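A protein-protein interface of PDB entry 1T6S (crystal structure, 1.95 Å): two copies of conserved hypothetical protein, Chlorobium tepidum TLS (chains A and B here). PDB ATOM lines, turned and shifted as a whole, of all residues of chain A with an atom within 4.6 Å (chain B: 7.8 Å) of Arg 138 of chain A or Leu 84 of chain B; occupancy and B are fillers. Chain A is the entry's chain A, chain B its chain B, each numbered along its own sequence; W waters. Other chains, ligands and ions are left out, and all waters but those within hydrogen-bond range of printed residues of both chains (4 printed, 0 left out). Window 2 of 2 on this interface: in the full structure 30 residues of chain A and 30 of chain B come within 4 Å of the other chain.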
ATOM      1  N   GLN A 107     -17.298 -13.041  14.786  1.00  0.00           N
ATOM      2  CA  GLN A 107     -18.422 -12.876  13.869  1.00  0.00           C
ATOM      3  C   GLN A 107     -18.080 -12.202  12.530  1.00  0.00           C
ATOM      4  O   GLN A 107     -17.260 -11.280  12.464  1.00  0.00           O
ATOM      5  CB  GLN A 107     -19.551 -12.096  14.559  1.00  0.00           C
ATOM      6  CG  GLN A 107     -19.155 -10.690  15.049  1.00  0.00           C
ATOM      7  CD  GLN A 107     -20.280 -10.000  15.811  1.00  0.00           C
ATOM      8  OE1 GLN A 107     -21.425  -9.987  15.366  1.00  0.00           O
ATOM      9  NE2 GLN A 107     -19.954  -9.418  16.959  1.00  0.00           N
ATOM     10  N   PRO A 108     -18.697 -12.676  11.431  1.00  0.00           N
ATOM     11  CA  PRO A 108     -19.666 -13.779  11.380  1.00  0.00           C
ATOM     12  C   PRO A 108     -18.914 -15.107  11.458  1.00  0.00           C
ATOM     13  O   PRO A 108     -17.920 -15.304  10.762  1.00  0.00           O
ATOM     14  CB  PRO A 108     -20.375 -13.554  10.040  1.00  0.00           C
ATOM     15  CG  PRO A 108     -19.333 -12.911   9.204  1.00  0.00           C
ATOM     16  CD  PRO A 108     -18.685 -11.937  10.155  1.00  0.00           C
ATOM     17  N   GLU A 136     -27.788 -13.979  16.275  1.00  0.00           N
ATOM     18  CA  GLU A 136     -28.683 -14.156  15.154  1.00  0.00           C
ATOM     19  C   GLU A 136     -27.857 -14.583  13.944  1.00  0.00           C
ATOM     20  O   GLU A 136     -26.624 -14.503  13.947  1.00  0.00           O
ATOM     21  CB  GLU A 136     -29.371 -12.828  14.835  1.00  0.00           C
ATOM     22  CG  GLU A 136     -28.372 -11.735  14.454  1.00  0.00           C
ATOM     23  CD  GLU A 136     -29.034 -10.408  14.183  1.00  0.00           C
ATOM     24  OE1 GLU A 136     -28.297  -9.416  13.966  1.00  0.00           O
ATOM     25  OE2 GLU A 136     -30.285 -10.363  14.186  1.00  0.00           O
ATOM     26  N   VAL A 137     -28.541 -15.019  12.892  1.00  0.00           N
ATOM     27  CA  VAL A 137     -27.855 -15.429  11.668  1.00  0.00           C
ATOM     28  C   VAL A 137     -27.439 -14.189  10.872  1.00  0.00           C
ATOM     29  O   VAL A 137     -28.222 -13.255  10.733  1.00  0.00           O
ATOM     30  CB  VAL A 137     -28.777 -16.306  10.783  1.00  0.00           C
ATOM     31  CG1 VAL A 137     -28.128 -16.548   9.413  1.00  0.00           C
ATOM     32  CG2 VAL A 137     -29.059 -17.622  11.474  1.00  0.00           C
ATOM     33  N   ARG A 138     -26.217 -14.188  10.347  1.00  0.00           N
ATOM     34  CA  ARG A 138     -25.707 -13.076   9.544  1.00  0.00           C
ATOM     35  C   ARG A 138     -25.605 -13.487   8.082  1.00  0.00           C
ATOM     36  O   ARG A 138     -25.379 -12.648   7.210  1.00  0.00           O
ATOM     37  CB  ARG A 138     -24.309 -12.668  10.002  1.00  0.00           C
ATOM     38  CG  ARG A 138     -24.254 -11.799  11.224  1.00  0.00           C
ATOM     39  CD  ARG A 138     -24.004 -10.335  10.851  1.00  0.00           C
ATOM     40  NE  ARG A 138     -23.421  -9.616  11.994  1.00  0.00           N
ATOM     41  CZ  ARG A 138     -24.081  -9.329  13.111  1.00  0.00           C
ATOM     42  NH1 ARG A 138     -25.356  -9.685  13.243  1.00  0.00           N
ATOM     43  NH2 ARG A 138     -23.457  -8.714  14.100  1.00  0.00           N
ATOM     44  N   GLY A 139     -25.744 -14.788   7.828  1.00  0.00           N
ATOM     45  CA  GLY A 139     -25.659 -15.310   6.474  1.00  0.00           C
ATOM     46  C   GLY A 139     -25.134 -16.737   6.453  1.00  0.00           C
ATOM     47  O   GLY A 139     -25.258 -17.445   7.445  1.00  0.00           O
ATOM     48  N   GLN A 149     -23.801 -18.618   9.576  1.00  0.00           N
ATOM     49  CA  GLN A 149     -22.826 -17.811  10.314  1.00  0.00           C
ATOM     50  C   GLN A 149     -23.617 -17.008  11.317  1.00  0.00           C
ATOM     51  O   GLN A 149     -24.734 -16.578  11.018  1.00  0.00           O
ATOM     52  CB  GLN A 149     -22.105 -16.840   9.382  1.00  0.00           C
ATOM     53  CG  GLN A 149     -21.329 -17.501   8.276  1.00  0.00           C
ATOM     54  CD  GLN A 149     -20.791 -16.485   7.304  1.00  0.00           C
ATOM     55  OE1 GLN A 149     -21.559 -15.768   6.661  1.00  0.00           O
ATOM     56  NE2 GLN A 149     -19.472 -16.402   7.202  1.00  0.00           N
ATOM     57  N   TYR A 150     -23.053 -16.794  12.499  1.00  0.00           N
ATOM     58  CA  TYR A 150     -23.754 -16.036  13.537  1.00  0.00           C
ATOM     59  C   TYR A 150     -23.050 -14.764  13.949  1.00  0.00           C
ATOM     60  O   TYR A 150     -21.848 -14.624  13.758  1.00  0.00           O
ATOM     61  CB  TYR A 150     -23.980 -16.905  14.773  1.00  0.00           C
ATOM     62  CG  TYR A 150     -24.749 -18.168  14.483  1.00  0.00           C
ATOM     63  CD1 TYR A 150     -24.103 -19.326  14.052  1.00  0.00           C
ATOM     64  CD2 TYR A 150     -26.133 -18.190  14.584  1.00  0.00           C
ATOM     65  CE1 TYR A 150     -24.834 -20.477  13.725  1.00  0.00           C
ATOM     66  CE2 TYR A 150     -26.857 -19.325  14.258  1.00  0.00           C
ATOM     67  CZ  TYR A 150     -26.204 -20.460  13.830  1.00  0.00           C
ATOM     68  OH  TYR A 150     -26.947 -21.565  13.496  1.00  0.00           O
ATOM     69  N   GLY A 151     -23.821 -13.838  14.510  1.00  0.00           N
ATOM     70  CA  GLY A 151     -23.271 -12.574  14.976  1.00  0.00           C
ATOM     71  C   GLY A 151     -24.097 -12.145  16.179  1.00  0.00           C
ATOM     72  O   GLY A 151     -25.163 -12.706  16.406  1.00  0.00           O
ATOM     73  N   THR A 152     -23.615 -11.177  16.954  1.00  0.00           N
ATOM     74  CA  THR A 152     -24.353 -10.707  18.119  1.00  0.00           C
ATOM     75  C   THR A 152     -25.507  -9.808  17.650  1.00  0.00           C
ATOM     76  O   THR A 152     -25.526  -9.378  16.499  1.00  0.00           O
ATOM     77  CB  THR A 152     -23.425  -9.922  19.104  1.00  0.00           C
ATOM     78  OG1 THR A 152     -22.683  -8.939  18.376  1.00  0.00           O
ATOM     79  CG2 THR A 152     -22.450 -10.882  19.812  1.00  0.00           C
ATOM     80  N   LEU A 157     -26.196  -6.005  22.600  1.00  0.00           N
ATOM     81  CA  LEU A 157     -25.505  -4.752  22.835  1.00  0.00           C
ATOM     82  C   LEU A 157     -26.242  -3.841  23.811  1.00  0.00           C
ATOM     83  O   LEU A 157     -25.624  -3.277  24.713  1.00  0.00           O
ATOM     84  CB  LEU A 157     -25.247  -4.034  21.504  1.00  0.00           C
ATOM     85  CG  LEU A 157     -24.323  -4.775  20.530  1.00  0.00           C
ATOM     86  CD1 LEU A 157     -24.225  -4.022  19.218  1.00  0.00           C
ATOM     87  CD2 LEU A 157     -22.920  -4.919  21.154  1.00  0.00           C
ATOM     88  N   HIS B  62     -34.063 -14.693   2.446  1.00  0.00           N
ATOM     89  CA  HIS B  62     -33.556 -16.034   2.705  1.00  0.00           C
ATOM     90  C   HIS B  62     -34.495 -16.857   3.592  1.00  0.00           C
ATOM     91  O   HIS B  62     -35.039 -16.369   4.601  1.00  0.00           O
ATOM     92  CB  HIS B  62     -32.193 -15.952   3.404  1.00  0.00           C
ATOM     93  CG  HIS B  62     -31.112 -15.346   2.567  1.00  0.00           C
ATOM     94  ND1 HIS B  62     -30.181 -16.106   1.892  1.00  0.00           N
ATOM     95  CD2 HIS B  62     -30.805 -14.055   2.298  1.00  0.00           C
ATOM     96  CE1 HIS B  62     -29.349 -15.309   1.246  1.00  0.00           C
ATOM     97  NE2 HIS B  62     -29.706 -14.061   1.476  1.00  0.00           N
ATOM     98  N   ARG B  69     -36.338 -14.013   6.075  1.00  0.00           N
ATOM     99  CA  ARG B  69     -35.817 -12.710   6.517  1.00  0.00           C
ATOM    100  C   ARG B  69     -34.876 -12.145   5.459  1.00  0.00           C
ATOM    101  O   ARG B  69     -34.299 -12.890   4.670  1.00  0.00           O
ATOM    102  CB  ARG B  69     -35.068 -12.828   7.854  1.00  0.00           C
ATOM    103  CG  ARG B  69     -33.618 -13.332   7.765  1.00  0.00           C
ATOM    104  CD  ARG B  69     -33.500 -14.741   7.189  1.00  0.00           C
ATOM    105  NE  ARG B  69     -34.173 -15.804   7.957  1.00  0.00           N
ATOM    106  CZ  ARG B  69     -33.876 -16.183   9.206  1.00  0.00           C
ATOM    107  NH1 ARG B  69     -32.914 -15.588   9.897  1.00  0.00           N
ATOM    108  NH2 ARG B  69     -34.507 -17.216   9.750  1.00  0.00           N
ATOM    109  N   PHE B  70     -34.741 -10.822   5.442  1.00  0.00           N
ATOM    110  CA  PHE B  70     -33.834 -10.144   4.522  1.00  0.00           C
ATOM    111  C   PHE B  70     -32.425 -10.226   5.072  1.00  0.00           C
ATOM    112  O   PHE B  70     -32.226 -10.229   6.288  1.00  0.00           O
ATOM    113  CB  PHE B  70     -34.192  -8.662   4.391  1.00  0.00           C
ATOM    114  CG  PHE B  70     -35.250  -8.379   3.373  1.00  0.00           C
ATOM    115  CD1 PHE B  70     -36.597  -8.391   3.725  1.00  0.00           C
ATOM    116  CD2 PHE B  70     -34.900  -8.122   2.044  1.00  0.00           C
ATOM    117  CE1 PHE B  70     -37.588  -8.152   2.775  1.00  0.00           C
ATOM    118  CE2 PHE B  70     -35.882  -7.880   1.082  1.00  0.00           C
ATOM    119  CZ  PHE B  70     -37.231  -7.895   1.447  1.00  0.00           C
ATOM    120  N   LEU B  71     -31.451 -10.301   4.174  1.00  0.00           N
ATOM    121  CA  LEU B  71     -30.035 -10.323   4.541  1.00  0.00           C
ATOM    122  C   LEU B  71     -29.307  -9.538   3.449  1.00  0.00           C
ATOM    123  O   LEU B  71     -29.712  -9.593   2.287  1.00  0.00           O
ATOM    124  CB  LEU B  71     -29.509 -11.760   4.594  1.00  0.00           C
ATOM    125  CG  LEU B  71     -28.992 -12.308   5.926  1.00  0.00           C
ATOM    126  CD1 LEU B  71     -29.960 -12.029   7.066  1.00  0.00           C
ATOM    127  CD2 LEU B  71     -28.776 -13.816   5.771  1.00  0.00           C
ATOM    128  N   THR B  72     -28.267  -8.787   3.804  1.00  0.00           N
ATOM    129  CA  THR B  72     -27.533  -8.033   2.786  1.00  0.00           C
ATOM    130  C   THR B  72     -26.576  -8.985   2.077  1.00  0.00           C
ATOM    131  O   THR B  72     -26.141  -9.980   2.656  1.00  0.00           O
ATOM    132  CB  THR B  72     -26.721  -6.816   3.358  1.00  0.00           C
ATOM    133  OG1 THR B  72     -25.973  -7.217   4.509  1.00  0.00           O
ATOM    134  CG2 THR B  72     -27.665  -5.666   3.741  1.00  0.00           C
ATOM    135  N   GLU B  73     -26.268  -8.670   0.824  1.00  0.00           N
ATOM    136  CA  GLU B  73     -25.383  -9.478  -0.009  1.00  0.00           C
ATOM    137  C   GLU B  73     -23.951  -9.567   0.525  1.00  0.00           C
ATOM    138  O   GLU B  73     -23.420  -8.599   1.076  1.00  0.00           O
ATOM    139  CB  GLU B  73     -25.378  -8.918  -1.435  1.00  0.00           C
ATOM    140  CG  GLU B  73     -26.686  -9.135  -2.163  1.00  0.00           C
ATOM    141  CD  GLU B  73     -26.851 -10.575  -2.626  1.00  0.00           C
ATOM    142  OE1 GLU B  73     -26.373 -10.889  -3.742  1.00  0.00           O
ATOM    143  OE2 GLU B  73     -27.438 -11.395  -1.873  1.00  0.00           O
ATOM    144  N   PRO B  74     -23.298 -10.734   0.344  1.00  0.00           N
ATOM    145  CA  PRO B  74     -21.922 -10.942   0.817  1.00  0.00           C
ATOM    146  C   PRO B  74     -20.937  -9.932   0.269  1.00  0.00           C
ATOM    147  O   PRO B  74     -19.867  -9.723   0.835  1.00  0.00           O
ATOM    148  CB  PRO B  74     -21.614 -12.377   0.378  1.00  0.00           C
ATOM    149  CG  PRO B  74     -22.456 -12.545  -0.850  1.00  0.00           C
ATOM    150  CD  PRO B  74     -23.766 -11.903  -0.427  1.00  0.00           C
ATOM    151  N   ALA B  77     -20.180  -7.521   2.958  1.00  0.00           N
ATOM    152  CA  ALA B  77     -19.909  -8.107   4.262  1.00  0.00           C
ATOM    153  C   ALA B  77     -18.914  -7.314   5.092  1.00  0.00           C
ATOM    154  O   ALA B  77     -19.100  -7.160   6.299  1.00  0.00           O
ATOM    155  CB  ALA B  77     -19.417  -9.546   4.096  1.00  0.00           C
ATOM    156  N   ASP B  78     -17.862  -6.800   4.461  1.00  0.00           N
ATOM    157  CA  ASP B  78     -16.868  -6.042   5.214  1.00  0.00           C
ATOM    158  C   ASP B  78     -17.451  -4.751   5.767  1.00  0.00           C
ATOM    159  O   ASP B  78     -17.163  -4.361   6.903  1.00  0.00           O
ATOM    160  CB  ASP B  78     -15.640  -5.732   4.351  1.00  0.00           C
ATOM    161  CG  ASP B  78     -14.582  -4.933   5.108  1.00  0.00           C
ATOM    162  OD1 ASP B  78     -14.544  -3.691   4.958  1.00  0.00           O
ATOM    163  OD2 ASP B  78     -13.798  -5.545   5.876  1.00  0.00           O
ATOM    164  N   LEU B  79     -18.267  -4.083   4.959  1.00  0.00           N
ATOM    165  CA  LEU B  79     -18.890  -2.834   5.395  1.00  0.00           C
ATOM    166  C   LEU B  79     -19.849  -3.098   6.546  1.00  0.00           C
ATOM    167  O   LEU B  79     -19.867  -2.359   7.534  1.00  0.00           O
ATOM    168  CB  LEU B  79     -19.649  -2.179   4.234  1.00  0.00           C
ATOM    169  CG  LEU B  79     -18.790  -1.729   3.046  1.00  0.00           C
ATOM    170  CD1 LEU B  79     -19.679  -1.070   1.976  1.00  0.00           C
ATOM    171  CD2 LEU B  79     -17.733  -0.765   3.518  1.00  0.00           C
ATOM    172  N   VAL B  80     -20.638  -4.160   6.422  1.00  0.00           N
ATOM    173  CA  VAL B  80     -21.597  -4.502   7.460  1.00  0.00           C
ATOM    174  C   VAL B  80     -20.885  -4.823   8.770  1.00  0.00           C
ATOM    175  O   VAL B  80     -21.357  -4.465   9.868  1.00  0.00           O
ATOM    176  CB  VAL B  80     -22.474  -5.690   7.015  1.00  0.00           C
ATOM    177  CG1 VAL B  80     -23.415  -6.116   8.138  1.00  0.00           C
ATOM    178  CG2 VAL B  80     -23.267  -5.278   5.796  1.00  0.00           C
ATOM    179  N   ARG B  81     -19.727  -5.467   8.652  1.00  0.00           N
ATOM    180  CA  ARG B  81     -18.955  -5.821   9.837  1.00  0.00           C
ATOM    181  C   ARG B  81     -18.522  -4.546  10.564  1.00  0.00           C
ATOM    182  O   ARG B  81     -18.632  -4.453  11.783  1.00  0.00           O
ATOM    183  CB  ARG B  81     -17.723  -6.663   9.456  1.00  0.00           C
ATOM    184  CG  ARG B  81     -17.322  -7.688  10.530  1.00  0.00           C
ATOM    185  CD  ARG B  81     -16.127  -8.542  10.083  1.00  0.00           C
ATOM    186  NE  ARG B  81     -14.851  -7.988  10.532  1.00  0.00           N
ATOM    187  CZ  ARG B  81     -13.992  -8.636  11.318  1.00  0.00           C
ATOM    188  NH1 ARG B  81     -14.283  -9.860  11.730  1.00  0.00           N
ATOM    189  NH2 ARG B  81     -12.852  -8.063  11.700  1.00  0.00           N
ATOM    190  N   GLN B  82     -18.045  -3.557   9.820  1.00  0.00           N
ATOM    191  CA  GLN B  82     -17.616  -2.313  10.451  1.00  0.00           C
ATOM    192  C   GLN B  82     -18.749  -1.561  11.137  1.00  0.00           C
ATOM    193  O   GLN B  82     -18.510  -0.749  12.029  1.00  0.00           O
ATOM    194  CB  GLN B  82     -16.957  -1.403   9.429  1.00  0.00           C
ATOM    195  CG  GLN B  82     -15.759  -2.029   8.769  1.00  0.00           C
ATOM    196  CD  GLN B  82     -15.209  -1.166   7.656  1.00  0.00           C
ATOM    197  OE1 GLN B  82     -15.108  -1.609   6.511  1.00  0.00           O
ATOM    198  NE2 GLN B  82     -14.854   0.070   7.983  1.00  0.00           N
ATOM    199  N   LEU B  83     -19.983  -1.837  10.724  1.00  0.00           N
ATOM    200  CA  LEU B  83     -21.143  -1.172  11.301  1.00  0.00           C
ATOM    201  C   LEU B  83     -21.712  -1.913  12.512  1.00  0.00           C
ATOM    202  O   LEU B  83     -21.918  -1.330  13.578  1.00  0.00           O
ATOM    203  CB  LEU B  83     -22.245  -1.034  10.244  1.00  0.00           C
ATOM    204  CG  LEU B  83     -23.590  -0.436  10.711  1.00  0.00           C
ATOM    205  CD1 LEU B  83     -23.386   1.027  11.115  1.00  0.00           C
ATOM    206  CD2 LEU B  83     -24.637  -0.517   9.588  1.00  0.00           C
ATOM    207  N   LEU B  84     -21.989  -3.199  12.331  1.00  0.00           N
ATOM    208  CA  LEU B  84     -22.577  -4.011  13.393  1.00  0.00           C
ATOM    209  C   LEU B  84     -21.593  -4.477  14.458  1.00  0.00           C
ATOM    210  O   LEU B  84     -21.972  -4.664  15.614  1.00  0.00           O
ATOM    211  CB  LEU B  84     -23.264  -5.248  12.792  1.00  0.00           C
ATOM    212  CG  LEU B  84     -24.529  -5.027  11.943  1.00  0.00           C
ATOM    213  CD1 LEU B  84     -24.221  -4.096  10.808  1.00  0.00           C
ATOM    214  CD2 LEU B  84     -25.045  -6.350  11.405  1.00  0.00           C
ATOM    215  N   ALA B  85     -20.337  -4.660  14.065  1.00  0.00           N
ATOM    216  CA  ALA B  85     -19.324  -5.154  14.984  1.00  0.00           C
ATOM    217  C   ALA B  85     -17.936  -4.556  14.781  1.00  0.00           C
ATOM    218  O   ALA B  85     -16.996  -5.266  14.418  1.00  0.00           O
ATOM    219  CB  ALA B  85     -19.248  -6.688  14.872  1.00  0.00           C
ATOM    220  N   PRO B  86     -17.782  -3.239  14.997  1.00  0.00           N
ATOM    221  CA  PRO B  86     -16.455  -2.638  14.818  1.00  0.00           C
ATOM    222  C   PRO B  86     -15.489  -3.235  15.860  1.00  0.00           C
ATOM    223  O   PRO B  86     -15.931  -3.703  16.910  1.00  0.00           O
ATOM    224  CB  PRO B  86     -16.724  -1.146  15.027  1.00  0.00           C
ATOM    225  CG  PRO B  86     -17.869  -1.138  15.989  1.00  0.00           C
ATOM    226  CD  PRO B  86     -18.760  -2.243  15.450  1.00  0.00           C
ATOM    227  N   VAL B  87     -14.187  -3.216  15.564  1.00  0.00           N
ATOM    228  CA  VAL B  87     -13.152  -3.783  16.443  1.00  0.00           C
ATOM    229  C   VAL B  87     -13.224  -3.380  17.919  1.00  0.00           C
ATOM    230  O   VAL B  87     -13.179  -4.238  18.805  1.00  0.00           O
ATOM    231  CB  VAL B  87     -11.719  -3.424  15.962  1.00  0.00           C
ATOM    232  CG1 VAL B  87     -10.696  -4.354  16.633  1.00  0.00           C
ATOM    233  CG2 VAL B  87     -11.628  -3.516  14.449  1.00  0.00           C
ATOM    234  N   GLN B  89     -15.706  -2.148  19.634  1.00  0.00           N
ATOM    235  CA  GLN B  89     -16.918  -2.664  20.250  1.00  0.00           C
ATOM    236  C   GLN B  89     -16.712  -4.149  20.572  1.00  0.00           C
ATOM    237  O   GLN B  89     -17.104  -4.617  21.641  1.00  0.00           O
ATOM    238  CB  GLN B  89     -18.102  -2.491  19.291  1.00  0.00           C
ATOM    239  CG  GLN B  89     -19.423  -3.004  19.813  1.00  0.00           C
ATOM    240  CD  GLN B  89     -20.483  -3.019  18.725  1.00  0.00           C
ATOM    241  OE1 GLN B  89     -20.884  -1.960  18.222  1.00  0.00           O
ATOM    242  NE2 GLN B  89     -20.935  -4.222  18.344  1.00  0.00           N
ATOM    243  N   ARG B  90     -16.075  -4.877  19.654  1.00  0.00           N
ATOM    244  CA  ARG B  90     -15.824  -6.302  19.853  1.00  0.00           C
ATOM    245  C   ARG B  90     -14.896  -6.543  21.057  1.00  0.00           C
ATOM    246  O   ARG B  90     -15.108  -7.477  21.822  1.00  0.00           O
ATOM    247  CB  ARG B  90     -15.224  -6.917  18.575  1.00  0.00           C
ATOM    248  CG  ARG B  90     -16.257  -7.202  17.485  1.00  0.00           C
ATOM    249  CD  ARG B  90     -15.627  -7.137  16.110  1.00  0.00           C
ATOM    250  NE  ARG B  90     -14.486  -8.028  15.998  1.00  0.00           N
ATOM    251  CZ  ARG B  90     -13.422  -7.797  15.238  1.00  0.00           C
ATOM    252  NH1 ARG B  90     -13.349  -6.686  14.515  1.00  0.00           N
ATOM    253  NH2 ARG B  90     -12.431  -8.686  15.196  1.00  0.00           N
HETATM  254  O   HOH W   1     -30.902 -13.557  10.771  1.00  0.00           O
HETATM  255  O   HOH W   2     -15.452  -9.958  14.146  1.00  0.00           O
HETATM  256  O   HOH W   3     -23.285  -7.113  16.351  1.00  0.00           O
HETATM  257  O   HOH W   4     -31.571 -15.095  12.900  1.00  0.00           O
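Among the printed residues, pairs that only touch across the chains: Gln 107 of chain A with Ala 85 of chain B (3.5 Å), Arg 138 of chain A with Leu 71 of chain B (3.8 Å), Arg 138 of chain A with Leu 84 of chain B (3.6 Å), Gly 139 of chain A with Leu 71 of chain B (3.5 Å) and Leu 157 of chain A with Gln 89 of chain B (3.4 Å).
No position is printed for both chains.
O of Gln 107 of chain A lies within hydrogen-bond range of NH1 of Arg 81 of chain B (3.4 Å).
OE1 of Gln 107 of chain A sits at hydrogen-bond distance from NH2 of Arg 138 of chain A, 2.7 Å away. The backbone NH (N) of Thr 152 of chain A sits at hydrogen-bond distance from the side-chain amide oxygen (OE1) of Gln 107 of chain A, 3.0 Å away. OE1 of Glu 136 of chain A is in salt-bridge range of NH1 of Arg 138 of chain A (3.0 Å). The backbone carbonyl oxygen (O) of Gln 149 of chain A sits at hydrogen-bond distance from the backbone NH (N) of Arg 138 of chain A, 2.9 Å away. NH2 of Arg 138 of chain A is in hydrogen-bond range of O of Thr 152 of chain A (3.2 Å). The side-chain amide nitrogen (NE2) of Gln 89 of chain B sits at hydrogen-bond distance from the backbone carbonyl oxygen (O) of Leu 84 of chain B (3.0 Å).
Water W2 lies within hydrogen-bond range of the guanidinium group (NH1) of Arg 81 of chain B, the backbone carbonyl oxygen (O) of Gln 107 of chain A and the guanidinium group (NE) of Arg 90 of chain B. Water W1 bridges the backbone carbonyl oxygen (O) of Val 137 of chain A (2.7 Å) and the guanidinium group (NH1) of Arg 69 of chain B (3.0 Å). Water W3 lies within hydrogen-bond range of the guanidinium group (NH2) of Arg 138 of chain A, the side-chain hydroxyl (OG1) of Thr 152 of chain A and the backbone carbonyl oxygen (O) of Leu 84 of chain B. Water W4 bridges N of Val 137 of chain A and NH1 of Arg 69 of chain B.
Of the 11 printed residues of chain A, 4 touch a printed residue of chain B. Hydrophobic or aromatic side chains of chain A that line the printed part of chain B: Leu 157. Among the printed residues, 6 pairs touch across the chains. Among the printed residues, no Asp or Glu carboxylate lies within 4 Å of a Lys or Arg side-chain nitrogen of the other chain.
Of the printed residues of chain B, Gln 107 of chain A touches Arg 81 (3.4 Å) and Ala 85 (3.5 Å). Printed residues of chain A within 4 Å of Leu 71 of chain B: Arg 138 (3.8 Å) and Gly 139 (3.5 Å). Leu 84 of chain B touches one residue of chain A. Printed residues of chain A within 4 Å of Ala 85 of chain B: Gln 107. Printed residues of chain A within 4 Å of Gln 89 of chain B: Leu 157. The nearest printed residue of chain B that does not touch Leu 157 of chain A is Leu 84 of chain B (4.3 Å).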
